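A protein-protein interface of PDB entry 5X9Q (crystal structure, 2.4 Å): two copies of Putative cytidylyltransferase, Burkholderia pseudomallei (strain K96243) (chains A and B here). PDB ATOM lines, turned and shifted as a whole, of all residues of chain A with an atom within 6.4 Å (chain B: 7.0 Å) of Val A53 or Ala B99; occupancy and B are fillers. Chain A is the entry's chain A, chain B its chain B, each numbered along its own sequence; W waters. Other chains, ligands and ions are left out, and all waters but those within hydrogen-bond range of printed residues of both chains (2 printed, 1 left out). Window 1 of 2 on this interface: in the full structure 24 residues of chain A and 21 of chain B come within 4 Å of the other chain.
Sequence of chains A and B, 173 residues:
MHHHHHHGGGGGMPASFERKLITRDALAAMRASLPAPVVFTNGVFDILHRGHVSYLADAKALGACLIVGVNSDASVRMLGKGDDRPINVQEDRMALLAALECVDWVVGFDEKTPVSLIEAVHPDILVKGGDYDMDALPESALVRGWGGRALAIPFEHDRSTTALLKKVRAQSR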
ATOM      1  N   LEU A  48       6.811   0.097  -2.382  1.00  0.00           N
ATOM      2  CA  LEU A  48       7.215   0.317  -0.998  1.00  0.00           C
ATOM      3  C   LEU A  48       8.715   0.270  -0.888  1.00  0.00           C
ATOM      4  O   LEU A  48       9.353  -0.646  -1.411  1.00  0.00           O
ATOM      5  CB  LEU A  48       6.610  -0.718  -0.052  1.00  0.00           C
ATOM      6  CG  LEU A  48       5.191  -0.549   0.466  1.00  0.00           C
ATOM      7  CD1 LEU A  48       4.898  -1.653   1.448  1.00  0.00           C
ATOM      8  CD2 LEU A  48       5.104   0.764   1.179  1.00  0.00           C
ATOM      9  N   HIS A  49       9.273   1.232  -0.166  1.00  0.00           N
ATOM     10  CA  HIS A  49      10.679   1.187   0.164  1.00  0.00           C
ATOM     11  C   HIS A  49      10.819   1.408   1.663  1.00  0.00           C
ATOM     12  O   HIS A  49       9.824   1.619   2.361  1.00  0.00           O
ATOM     13  CB  HIS A  49      11.474   2.232  -0.622  1.00  0.00           C
ATOM     14  CG  HIS A  49      10.938   3.619  -0.494  1.00  0.00           C
ATOM     15  ND1 HIS A  49      11.053   4.359   0.668  1.00  0.00           N
ATOM     16  CD2 HIS A  49      10.355   4.439  -1.403  1.00  0.00           C
ATOM     17  CE1 HIS A  49      10.511   5.550   0.486  1.00  0.00           C
ATOM     18  NE2 HIS A  49      10.079   5.626  -0.763  1.00  0.00           N
ATOM     19  N   ARG A  50      12.051   1.354   2.150  1.00  0.00           N
ATOM     20  CA  ARG A  50      12.307   1.397   3.578  1.00  0.00           C
ATOM     21  C   ARG A  50      11.870   2.704   4.248  1.00  0.00           C
ATOM     22  O   ARG A  50      11.485   2.706   5.416  1.00  0.00           O
ATOM     23  CB  ARG A  50      13.789   1.141   3.834  1.00  0.00           C
ATOM     24  CG  ARG A  50      14.115   0.979   5.289  1.00  0.00           C
ATOM     25  CD  ARG A  50      15.584   0.773   5.490  1.00  0.00           C
ATOM     26  NE  ARG A  50      15.849   0.424   6.873  1.00  0.00           N
ATOM     27  CZ  ARG A  50      16.972  -0.138   7.298  1.00  0.00           C
ATOM     28  NH1 ARG A  50      17.947  -0.407   6.433  1.00  0.00           N
ATOM     29  NH2 ARG A  50      17.119  -0.420   8.586  1.00  0.00           N
ATOM     30  N   GLY A  51      11.923   3.810   3.514  1.00  0.00           N
ATOM     31  CA  GLY A  51      11.479   5.092   4.047  1.00  0.00           C
ATOM     32  C   GLY A  51       9.989   5.090   4.331  1.00  0.00           C
ATOM     33  O   GLY A  51       9.540   5.594   5.354  1.00  0.00           O
ATOM     34  N   HIS A  52       9.228   4.491   3.424  1.00  0.00           N
ATOM     35  CA  HIS A  52       7.795   4.320   3.587  1.00  0.00           C
ATOM     36  C   HIS A  52       7.452   3.594   4.881  1.00  0.00           C
ATOM     37  O   HIS A  52       6.627   4.063   5.657  1.00  0.00           O
ATOM     38  CB  HIS A  52       7.229   3.527   2.419  1.00  0.00           C
ATOM     39  CG  HIS A  52       7.092   4.314   1.156  1.00  0.00           C
ATOM     40  ND1 HIS A  52       7.477   3.819  -0.068  1.00  0.00           N
ATOM     41  CD2 HIS A  52       6.583   5.546   0.920  1.00  0.00           C
ATOM     42  CE1 HIS A  52       7.208   4.709  -1.006  1.00  0.00           C
ATOM     43  NE2 HIS A  52       6.665   5.766  -0.432  1.00  0.00           N
ATOM     44  N   VAL A  53       8.071   2.442   5.121  1.00  0.00           N
ATOM     45  CA  VAL A  53       7.688   1.649   6.285  1.00  0.00           C
ATOM     46  C   VAL A  53       8.241   2.219   7.581  1.00  0.00           C
ATOM     47  O   VAL A  53       7.596   2.099   8.617  1.00  0.00           O
ATOM     48  CB  VAL A  53       8.091   0.153   6.132  1.00  0.00           C
ATOM     49  CG1 VAL A  53       7.353  -0.463   4.916  1.00  0.00           C
ATOM     50  CG2 VAL A  53       9.593  -0.020   6.023  1.00  0.00           C
ATOM     51  N   SER A  54       9.413   2.843   7.521  1.00  0.00           N
ATOM     52  CA  SER A  54      10.009   3.444   8.707  1.00  0.00           C
ATOM     53  C   SER A  54       9.074   4.548   9.186  1.00  0.00           C
ATOM     54  O   SER A  54       8.791   4.671  10.378  1.00  0.00           O
ATOM     55  CB  SER A  54      11.390   4.018   8.389  1.00  0.00           C
ATOM     56  OG  SER A  54      12.351   2.985   8.261  1.00  0.00           O
ATOM     57  N   TYR A  55       8.573   5.344   8.254  1.00  0.00           N
ATOM     58  CA  TYR A  55       7.664   6.421   8.548  1.00  0.00           C
ATOM     59  C   TYR A  55       6.277   5.922   8.872  1.00  0.00           C
ATOM     60  O   TYR A  55       5.618   6.532   9.663  1.00  0.00           O
ATOM     61  CB  TYR A  55       7.688   7.500   7.453  1.00  0.00           C
ATOM     62  CG  TYR A  55       6.389   7.820   6.771  1.00  0.00           C
ATOM     63  CD1 TYR A  55       5.429   8.593   7.372  1.00  0.00           C
ATOM     64  CD2 TYR A  55       6.125   7.327   5.545  1.00  0.00           C
ATOM     65  CE1 TYR A  55       4.228   8.856   6.747  1.00  0.00           C
ATOM     66  CE2 TYR A  55       4.952   7.593   4.900  1.00  0.00           C
ATOM     67  CZ  TYR A  55       4.009   8.345   5.502  1.00  0.00           C
ATOM     68  OH  TYR A  55       2.874   8.547   4.803  1.00  0.00           O
ATOM     69  N   LEU A  56       5.854   4.822   8.257  1.00  0.00           N
ATOM     70  CA  LEU A  56       4.534   4.278   8.575  1.00  0.00           C
ATOM     71  C   LEU A  56       4.485   3.781  10.024  1.00  0.00           C
ATOM     72  O   LEU A  56       3.452   3.859  10.689  1.00  0.00           O
ATOM     73  CB  LEU A  56       4.176   3.143   7.614  1.00  0.00           C
ATOM     74  CG  LEU A  56       3.596   3.558   6.261  1.00  0.00           C
ATOM     75  CD1 LEU A  56       3.076   2.345   5.503  1.00  0.00           C
ATOM     76  CD2 LEU A  56       2.497   4.594   6.441  1.00  0.00           C
ATOM     77  N   ALA A  57       5.619   3.272  10.495  1.00  0.00           N
ATOM     78  CA  ALA A  57       5.784   2.747  11.850  1.00  0.00           C
ATOM     79  C   ALA A  57       5.838   3.844  12.901  1.00  0.00           C
ATOM     80  O   ALA A  57       5.172   3.736  13.926  1.00  0.00           O
ATOM     81  CB  ALA A  57       7.026   1.852  11.928  1.00  0.00           C
ATOM     82  N   ASP A  58       6.562   4.918  12.604  1.00  0.00           N
ATOM     83  CA  ASP A  58       6.646   6.054  13.509  1.00  0.00           C
ATOM     84  C   ASP A  58       5.288   6.755  13.641  1.00  0.00           C
ATOM     85  O   ASP A  58       4.927   7.209  14.729  1.00  0.00           O
ATOM     86  CB  ASP A  58       7.706   7.047  13.027  1.00  0.00           C
ATOM     87  CG  ASP A  58       9.117   6.585  13.329  1.00  0.00           C
ATOM     88  OD1 ASP A  58       9.278   5.652  14.143  1.00  0.00           O
ATOM     89  OD2 ASP A  58      10.067   7.154  12.750  1.00  0.00           O
ATOM     90  N   ALA A  99      -0.674  -5.366   4.509  1.00  0.00           N
ATOM     91  CA  ALA A  99       0.175  -6.459   4.982  1.00  0.00           C
ATOM     92  C   ALA A  99       1.104  -5.988   6.085  1.00  0.00           C
ATOM     93  O   ALA A  99       1.736  -6.806   6.766  1.00  0.00           O
ATOM     94  CB  ALA A  99       0.977  -7.053   3.837  1.00  0.00           C
ATOM     95  N   LEU A 100       1.175  -4.674   6.264  1.00  0.00           N
ATOM     96  CA  LEU A 100       2.081  -4.078   7.234  1.00  0.00           C
ATOM     97  C   LEU A 100       1.549  -4.171   8.662  1.00  0.00           C
ATOM     98  O   LEU A 100       0.368  -3.910   8.929  1.00  0.00           O
ATOM     99  CB  LEU A 100       2.322  -2.613   6.871  1.00  0.00           C
ATOM    100  CG  LEU A 100       3.046  -2.450   5.538  1.00  0.00           C
ATOM    101  CD1 LEU A 100       3.152  -0.988   5.141  1.00  0.00           C
ATOM    102  CD2 LEU A 100       4.431  -3.110   5.639  1.00  0.00           C
ATOM    103  N   GLU A 101       2.440  -4.528   9.578  1.00  0.00           N
ATOM    104  CA  GLU A 101       2.079  -4.656  10.980  1.00  0.00           C
ATOM    105  C   GLU A 101       1.550  -3.358  11.564  1.00  0.00           C
ATOM    106  O   GLU A 101       0.634  -3.371  12.376  1.00  0.00           O
ATOM    107  CB  GLU A 101       3.273  -5.109  11.816  1.00  0.00           C
ATOM    108  CG  GLU A 101       2.880  -5.348  13.271  1.00  0.00           C
ATOM    109  CD  GLU A 101       3.981  -5.988  14.087  1.00  0.00           C
ATOM    110  OE1 GLU A 101       5.168  -5.852  13.705  1.00  0.00           O
ATOM    111  OE2 GLU A 101       3.659  -6.666  15.093  1.00  0.00           O
ATOM    112  N   CYS A 102       2.140  -2.235  11.181  1.00  0.00           N
ATOM    113  CA  CYS A 102       1.786  -0.997  11.860  1.00  0.00           C
ATOM    114  C   CYS A 102       0.513  -0.337  11.355  1.00  0.00           C
ATOM    115  O   CYS A 102      -0.005   0.541  12.028  1.00  0.00           O
ATOM    116  CB  CYS A 102       2.941  -0.007  11.771  1.00  0.00           C
ATOM    117  SG  CYS A 102       3.324   0.520  10.109  1.00  0.00           S
ATOM    118  N   ALA B  15      10.636   0.919  13.409  1.00  0.00           N
ATOM    119  CA  ALA B  15      11.627   0.817  14.471  1.00  0.00           C
ATOM    120  C   ALA B  15      11.295  -0.331  15.428  1.00  0.00           C
ATOM    121  O   ALA B  15      12.169  -1.072  15.864  1.00  0.00           O
ATOM    122  CB  ALA B  15      11.711   2.133  15.222  1.00  0.00           C
ATOM    123  N   PHE B  17       9.445  -2.815  14.440  1.00  0.00           N
ATOM    124  CA  PHE B  17       9.540  -3.965  13.538  1.00  0.00           C
ATOM    125  C   PHE B  17      10.945  -4.546  13.378  1.00  0.00           C
ATOM    126  O   PHE B  17      11.104  -5.705  12.995  1.00  0.00           O
ATOM    127  CB  PHE B  17       8.969  -3.608  12.162  1.00  0.00           C
ATOM    128  CG  PHE B  17       9.748  -2.546  11.439  1.00  0.00           C
ATOM    129  CD1 PHE B  17      10.998  -2.826  10.909  1.00  0.00           C
ATOM    130  CD2 PHE B  17       9.232  -1.270  11.288  1.00  0.00           C
ATOM    131  CE1 PHE B  17      11.717  -1.853  10.242  1.00  0.00           C
ATOM    132  CE2 PHE B  17       9.946  -0.293  10.623  1.00  0.00           C
ATOM    133  CZ  PHE B  17      11.191  -0.584  10.100  1.00  0.00           C
ATOM    134  N   GLU B  18      11.955  -3.731  13.665  1.00  0.00           N
ATOM    135  CA  GLU B  18      13.346  -4.155  13.545  1.00  0.00           C
ATOM    136  C   GLU B  18      13.720  -5.196  14.593  1.00  0.00           C
ATOM    137  O   GLU B  18      14.819  -5.752  14.562  1.00  0.00           O
ATOM    138  CB  GLU B  18      14.282  -2.948  13.646  1.00  0.00           C
ATOM    139  CG  GLU B  18      14.176  -1.979  12.480  1.00  0.00           C
ATOM    140  CD  GLU B  18      15.458  -1.204  12.247  1.00  0.00           C
ATOM    141  OE1 GLU B  18      15.801  -0.349  13.092  1.00  0.00           O
ATOM    142  OE2 GLU B  18      16.124  -1.450  11.220  1.00  0.00           O
ATOM    143  N   LYS B  20      12.587  -7.910  14.698  1.00  0.00           N
ATOM    144  CA  LYS B  20      12.654  -9.151  13.954  1.00  0.00           C
ATOM    145  C   LYS B  20      13.934  -9.478  13.191  1.00  0.00           C
ATOM    146  O   LYS B  20      14.155 -10.626  12.839  1.00  0.00           O
ATOM    147  CB  LYS B  20      11.457  -9.146  12.999  1.00  0.00           C
ATOM    148  CG  LYS B  20      10.111  -8.881  13.668  1.00  0.00           C
ATOM    149  CD  LYS B  20       8.983  -8.964  12.635  1.00  0.00           C
ATOM    150  CE  LYS B  20       7.678  -8.479  13.209  1.00  0.00           C
ATOM    151  NZ  LYS B  20       6.619  -8.529  12.145  1.00  0.00           N
ATOM    152  N   ASP B  92      17.879  -3.414   3.532  1.00  0.00           N
ATOM    153  CA  ASP B  92      16.610  -2.803   3.140  1.00  0.00           C
ATOM    154  C   ASP B  92      15.587  -3.885   2.797  1.00  0.00           C
ATOM    155  O   ASP B  92      14.394  -3.755   3.107  1.00  0.00           O
ATOM    156  CB  ASP B  92      16.780  -1.856   1.941  1.00  0.00           C
ATOM    157  CG  ASP B  92      17.399  -0.507   2.329  1.00  0.00           C
ATOM    158  OD1 ASP B  92      17.964  -0.407   3.443  1.00  0.00           O
ATOM    159  OD2 ASP B  92      17.267   0.469   1.542  1.00  0.00           O
ATOM    160  N   MET B  94      15.600  -6.855   4.038  1.00  0.00           N
ATOM    161  CA  MET B  94      15.248  -7.502   5.293  1.00  0.00           C
ATOM    162  C   MET B  94      14.284  -6.622   6.110  1.00  0.00           C
ATOM    163  O   MET B  94      13.313  -7.118   6.699  1.00  0.00           O
ATOM    164  CB  MET B  94      16.500  -7.809   6.108  1.00  0.00           C
ATOM    165  CG  MET B  94      17.394  -8.880   5.523  1.00  0.00           C
ATOM    166  SD  MET B  94      18.891  -9.115   6.530  1.00  0.00           S
ATOM    167  CE  MET B  94      18.233  -9.910   8.000  1.00  0.00           C
ATOM    168  N   ALA B  95      14.535  -5.317   6.121  1.00  0.00           N
ATOM    169  CA  ALA B  95      13.646  -4.373   6.804  1.00  0.00           C
ATOM    170  C   ALA B  95      12.225  -4.386   6.221  1.00  0.00           C
ATOM    171  O   ALA B  95      11.251  -4.326   6.962  1.00  0.00           O
ATOM    172  CB  ALA B  95      14.220  -2.959   6.740  1.00  0.00           C
ATOM    173  N   LEU B  96      12.104  -4.450   4.900  1.00  0.00           N
ATOM    174  CA  LEU B  96      10.789  -4.485   4.270  1.00  0.00           C
ATOM    175  C   LEU B  96       9.995  -5.687   4.765  1.00  0.00           C
ATOM    176  O   LEU B  96       8.845  -5.562   5.195  1.00  0.00           O
ATOM    177  CB  LEU B  96      10.929  -4.506   2.742  1.00  0.00           C
ATOM    178  CG  LEU B  96      10.699  -3.134   2.105  1.00  0.00           C
ATOM    179  CD1 LEU B  96       9.217  -2.823   2.024  1.00  0.00           C
ATOM    180  CD2 LEU B  96      11.411  -2.037   2.904  1.00  0.00           C
ATOM    181  N   LEU B  97      10.638  -6.849   4.737  1.00  0.00           N
ATOM    182  CA  LEU B  97      10.027  -8.076   5.227  1.00  0.00           C
ATOM    183  C   LEU B  97       9.649  -7.996   6.697  1.00  0.00           C
ATOM    184  O   LEU B  97       8.570  -8.446   7.091  1.00  0.00           O
ATOM    185  CB  LEU B  97      10.980  -9.261   5.003  1.00  0.00           C
ATOM    186  CG  LEU B  97      11.076  -9.645   3.538  1.00  0.00           C
ATOM    187  CD1 LEU B  97      12.301 -10.470   3.259  1.00  0.00           C
ATOM    188  CD2 LEU B  97       9.825 -10.386   3.144  1.00  0.00           C
ATOM    189  N   ALA B  98      10.531  -7.422   7.513  1.00  0.00           N
ATOM    190  CA  ALA B  98      10.292  -7.391   8.954  1.00  0.00           C
ATOM    191  C   ALA B  98       9.063  -6.538   9.282  1.00  0.00           C
ATOM    192  O   ALA B  98       8.430  -6.715  10.326  1.00  0.00           O
ATOM    193  CB  ALA B  98      11.518  -6.870   9.686  1.00  0.00           C
ATOM    194  N   ALA B  99       8.743  -5.603   8.393  1.00  0.00           N
ATOM    195  CA  ALA B  99       7.582  -4.730   8.564  1.00  0.00           C
ATOM    196  C   ALA B  99       6.278  -5.468   8.309  1.00  0.00           C
ATOM    197  O   ALA B  99       5.207  -4.957   8.611  1.00  0.00           O
ATOM    198  CB  ALA B  99       7.686  -3.527   7.639  1.00  0.00           C
ATOM    199  N   LEU B 100       6.351  -6.670   7.747  1.00  0.00           N
ATOM    200  CA  LEU B 100       5.122  -7.382   7.435  1.00  0.00           C
ATOM    201  C   LEU B 100       4.534  -8.008   8.682  1.00  0.00           C
ATOM    202  O   LEU B 100       5.250  -8.590   9.495  1.00  0.00           O
ATOM    203  CB  LEU B 100       5.357  -8.450   6.362  1.00  0.00           C
ATOM    204  CG  LEU B 100       5.710  -7.857   4.992  1.00  0.00           C
ATOM    205  CD1 LEU B 100       5.989  -8.961   3.996  1.00  0.00           C
ATOM    206  CD2 LEU B 100       4.589  -6.952   4.495  1.00  0.00           C
ATOM    207  N   GLU B 101       3.218  -7.903   8.817  1.00  0.00           N
ATOM    208  CA  GLU B 101       2.537  -8.439   9.992  1.00  0.00           C
ATOM    209  C   GLU B 101       2.800  -9.940  10.185  1.00  0.00           C
ATOM    210  O   GLU B 101       2.995 -10.418  11.299  1.00  0.00           O
ATOM    211  CB  GLU B 101       1.031  -8.214   9.864  1.00  0.00           C
ATOM    212  CG  GLU B 101       0.222  -8.608  11.104  1.00  0.00           C
ATOM    213  CD  GLU B 101      -1.253  -8.233  10.965  1.00  0.00           C
ATOM    214  OE1 GLU B 101      -1.732  -8.096   9.813  1.00  0.00           O
ATOM    215  OE2 GLU B 101      -1.935  -8.073  12.006  1.00  0.00           O
ATOM    216  N   CYS B 102       2.818 -10.681   9.086  1.00  0.00           N
ATOM    217  CA  CYS B 102       2.850 -12.128   9.181  1.00  0.00           C
ATOM    218  C   CYS B 102       4.255 -12.705   9.431  1.00  0.00           C
ATOM    219  O   CYS B 102       4.388 -13.897   9.701  1.00  0.00           O
ATOM    220  CB  CYS B 102       2.262 -12.731   7.903  1.00  0.00           C
ATOM    221  SG  CYS B 102       3.280 -12.428   6.478  1.00  0.00           S
ATOM    222  N   VAL B 103       5.290 -11.877   9.309  1.00  0.00           N
ATOM    223  CA  VAL B 103       6.672 -12.324   9.430  1.00  0.00           C
ATOM    224  C   VAL B 103       7.137 -12.249  10.876  1.00  0.00           C
ATOM    225  O   VAL B 103       6.893 -11.237  11.537  1.00  0.00           O
ATOM    226  CB  VAL B 103       7.610 -11.466   8.551  1.00  0.00           C
ATOM    227  CG1 VAL B 103       9.057 -11.799   8.814  1.00  0.00           C
ATOM    228  CG2 VAL B 103       7.302 -11.664   7.079  1.00  0.00           C
ATOM    229  N   VAL B 106      13.550 -12.353  10.529  1.00  0.00           N
ATOM    230  CA  VAL B 106      14.237 -12.227   9.243  1.00  0.00           C
ATOM    231  C   VAL B 106      15.742 -12.404   9.469  1.00  0.00           C
ATOM    232  O   VAL B 106      16.327 -11.696  10.305  1.00  0.00           O
ATOM    233  CB  VAL B 106      13.952 -10.872   8.576  1.00  0.00           C
ATOM    234  CG1 VAL B 106      14.531 -10.836   7.177  1.00  0.00           C
ATOM    235  CG2 VAL B 106      12.444 -10.593   8.537  1.00  0.00           C
HETATM  236  O   HOH W   1       4.833  -2.163  10.261  1.00  0.00           O
HETATM  237  O   HOH W   2       1.453  -9.592   6.745  1.00  0.00           O
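NZ of Lys B20 lies within salt-bridge range of OE1 of Glu A101 (3.4 Å).
The guanidinium group of Arg A50 lies within salt-bridge range of the side-chain carboxylate of Asp B92, at 3.0 Å.
The side-chain carboxylate (OE2) of Glu B18 lies within salt-bridge range of the guanidinium group (NH2) of Arg A50 (3.0 Å).
The backbone NH (N) of Glu B101 sits at hydrogen-bond distance from the backbone carbonyl oxygen (O) of Ala A99, 2.8 Å away.
The backbone NH (N) of Glu A101 sits at hydrogen-bond distance from the backbone carbonyl oxygen (O) of Ala B99 (3.0 Å).
The side-chain amino group (NZ) of Lys B20 lies within hydrogen-bond range of the backbone carbonyl oxygen (O) of Ala B98 (3.1 Å).
ND1 of His A52 sits at hydrogen-bond distance from N of His A49, at 3.2 Å.
N of Gly A51 is in hydrogen-bond range of ND1 of His A49, at 3.0 Å.
The backbone carbonyl oxygen (O) of Lys B20 sits at hydrogen-bond distance from the backbone NH (N) of Val B106, 2.9 Å away.
The side-chain amino group of Lys B20 lies within hydrogen-bond range of the backbone carbonyl oxygen of Leu B100 (3.0 Å).
The backbone carbonyl oxygen of Arg A50 lies within hydrogen-bond range of the side-chain hydroxyl of Ser A54 (3.0 Å).
Among the printed residues, merely in contact across the chains: Leu A48 with Leu B96 (3.9 Å), His A49 with Leu B96 (3.7 Å), Arg A50 with Ala B95 (3.8 Å), Arg A50 with Leu B96 (3.5 Å), Val A53 with Phe B17 (3.9 Å), Val A53 with Ala B99 (3.997 Å), Ala A57 with Phe B17 (3.9 Å), Ala A99 with Leu B100 (3.5 Å), Leu A100 with Ala B99 (3.5 Å) and Glu A101 with Glu B101 (3.5 Å).
Of the printed residues of chain B, Leu A48 touches Leu B96 (3.9 Å).
Of the printed residues of chain B, Val A53 touches Phe B17 and Ala B99.
Leu A56 touches none of the printed residues of chain B.
Printed residues of chain A within 4 Å of Lys B20: Glu A101 (3.4 Å).
Of the printed residues of chain A, Ala B95 touches Arg A50 (3.8 Å).
Of the printed residues of chain A, Leu B96 touches Leu A48 (3.9 Å), His A49 (3.7 Å) and Arg A50 (3.5 Å).
Printed residues of chain A within 4 Å of Ala B99: Val A53 (3.997 Å), Leu A100 (3.5 Å) and Glu A101 (3.0 Å).
The nearest printed residue of chain A that does not touch Ala B99 is Ala A99 (4.3 Å).
The nearest printed residue of chain B that does not touch Glu A101 is Leu B100 (4.2 Å).
Printed residues of chain B that touch a printed residue of chain A: Phe B17, Glu B18, Lys B20, Asp B92, Ala B95, Leu B96, Ala B99, Leu B100 and Glu B101.
Hydrophobic or aromatic side chains of chain A that line the printed part of chain B: Leu A48, Val A53, Ala A57, Ala A99 and Leu A100.
Among the printed residues, 15 pairs touch across the chains.
Among the printed residues, Asp or Glu carboxylates within 4 Å of a Lys or Arg side-chain nitrogen of the other chain: Arg A50 with Glu B18, Arg A50 with Asp B92 and Glu A101 with Lys B20.
Ala A99 touches Leu B100, and with the chains exchanged Leu A100 touches Ala B99.
Ala A99 touches Glu B101, and with the chains exchanged Glu A101 touches Ala B99.
Glu A101 touches its own counterpart, Glu B101.
4 positions are printed for both chains.
Water W2 lies within hydrogen-bond range of the backbone carbonyl oxygen of Ala A99, the backbone NH of Cys B102 and the backbone NH of Glu B101.
Water W1 lies within hydrogen-bond range of N of Cys A102 (2.8 Å), O of Ala B99 (3.3 Å) and N of Glu A101 (3.4 Å).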
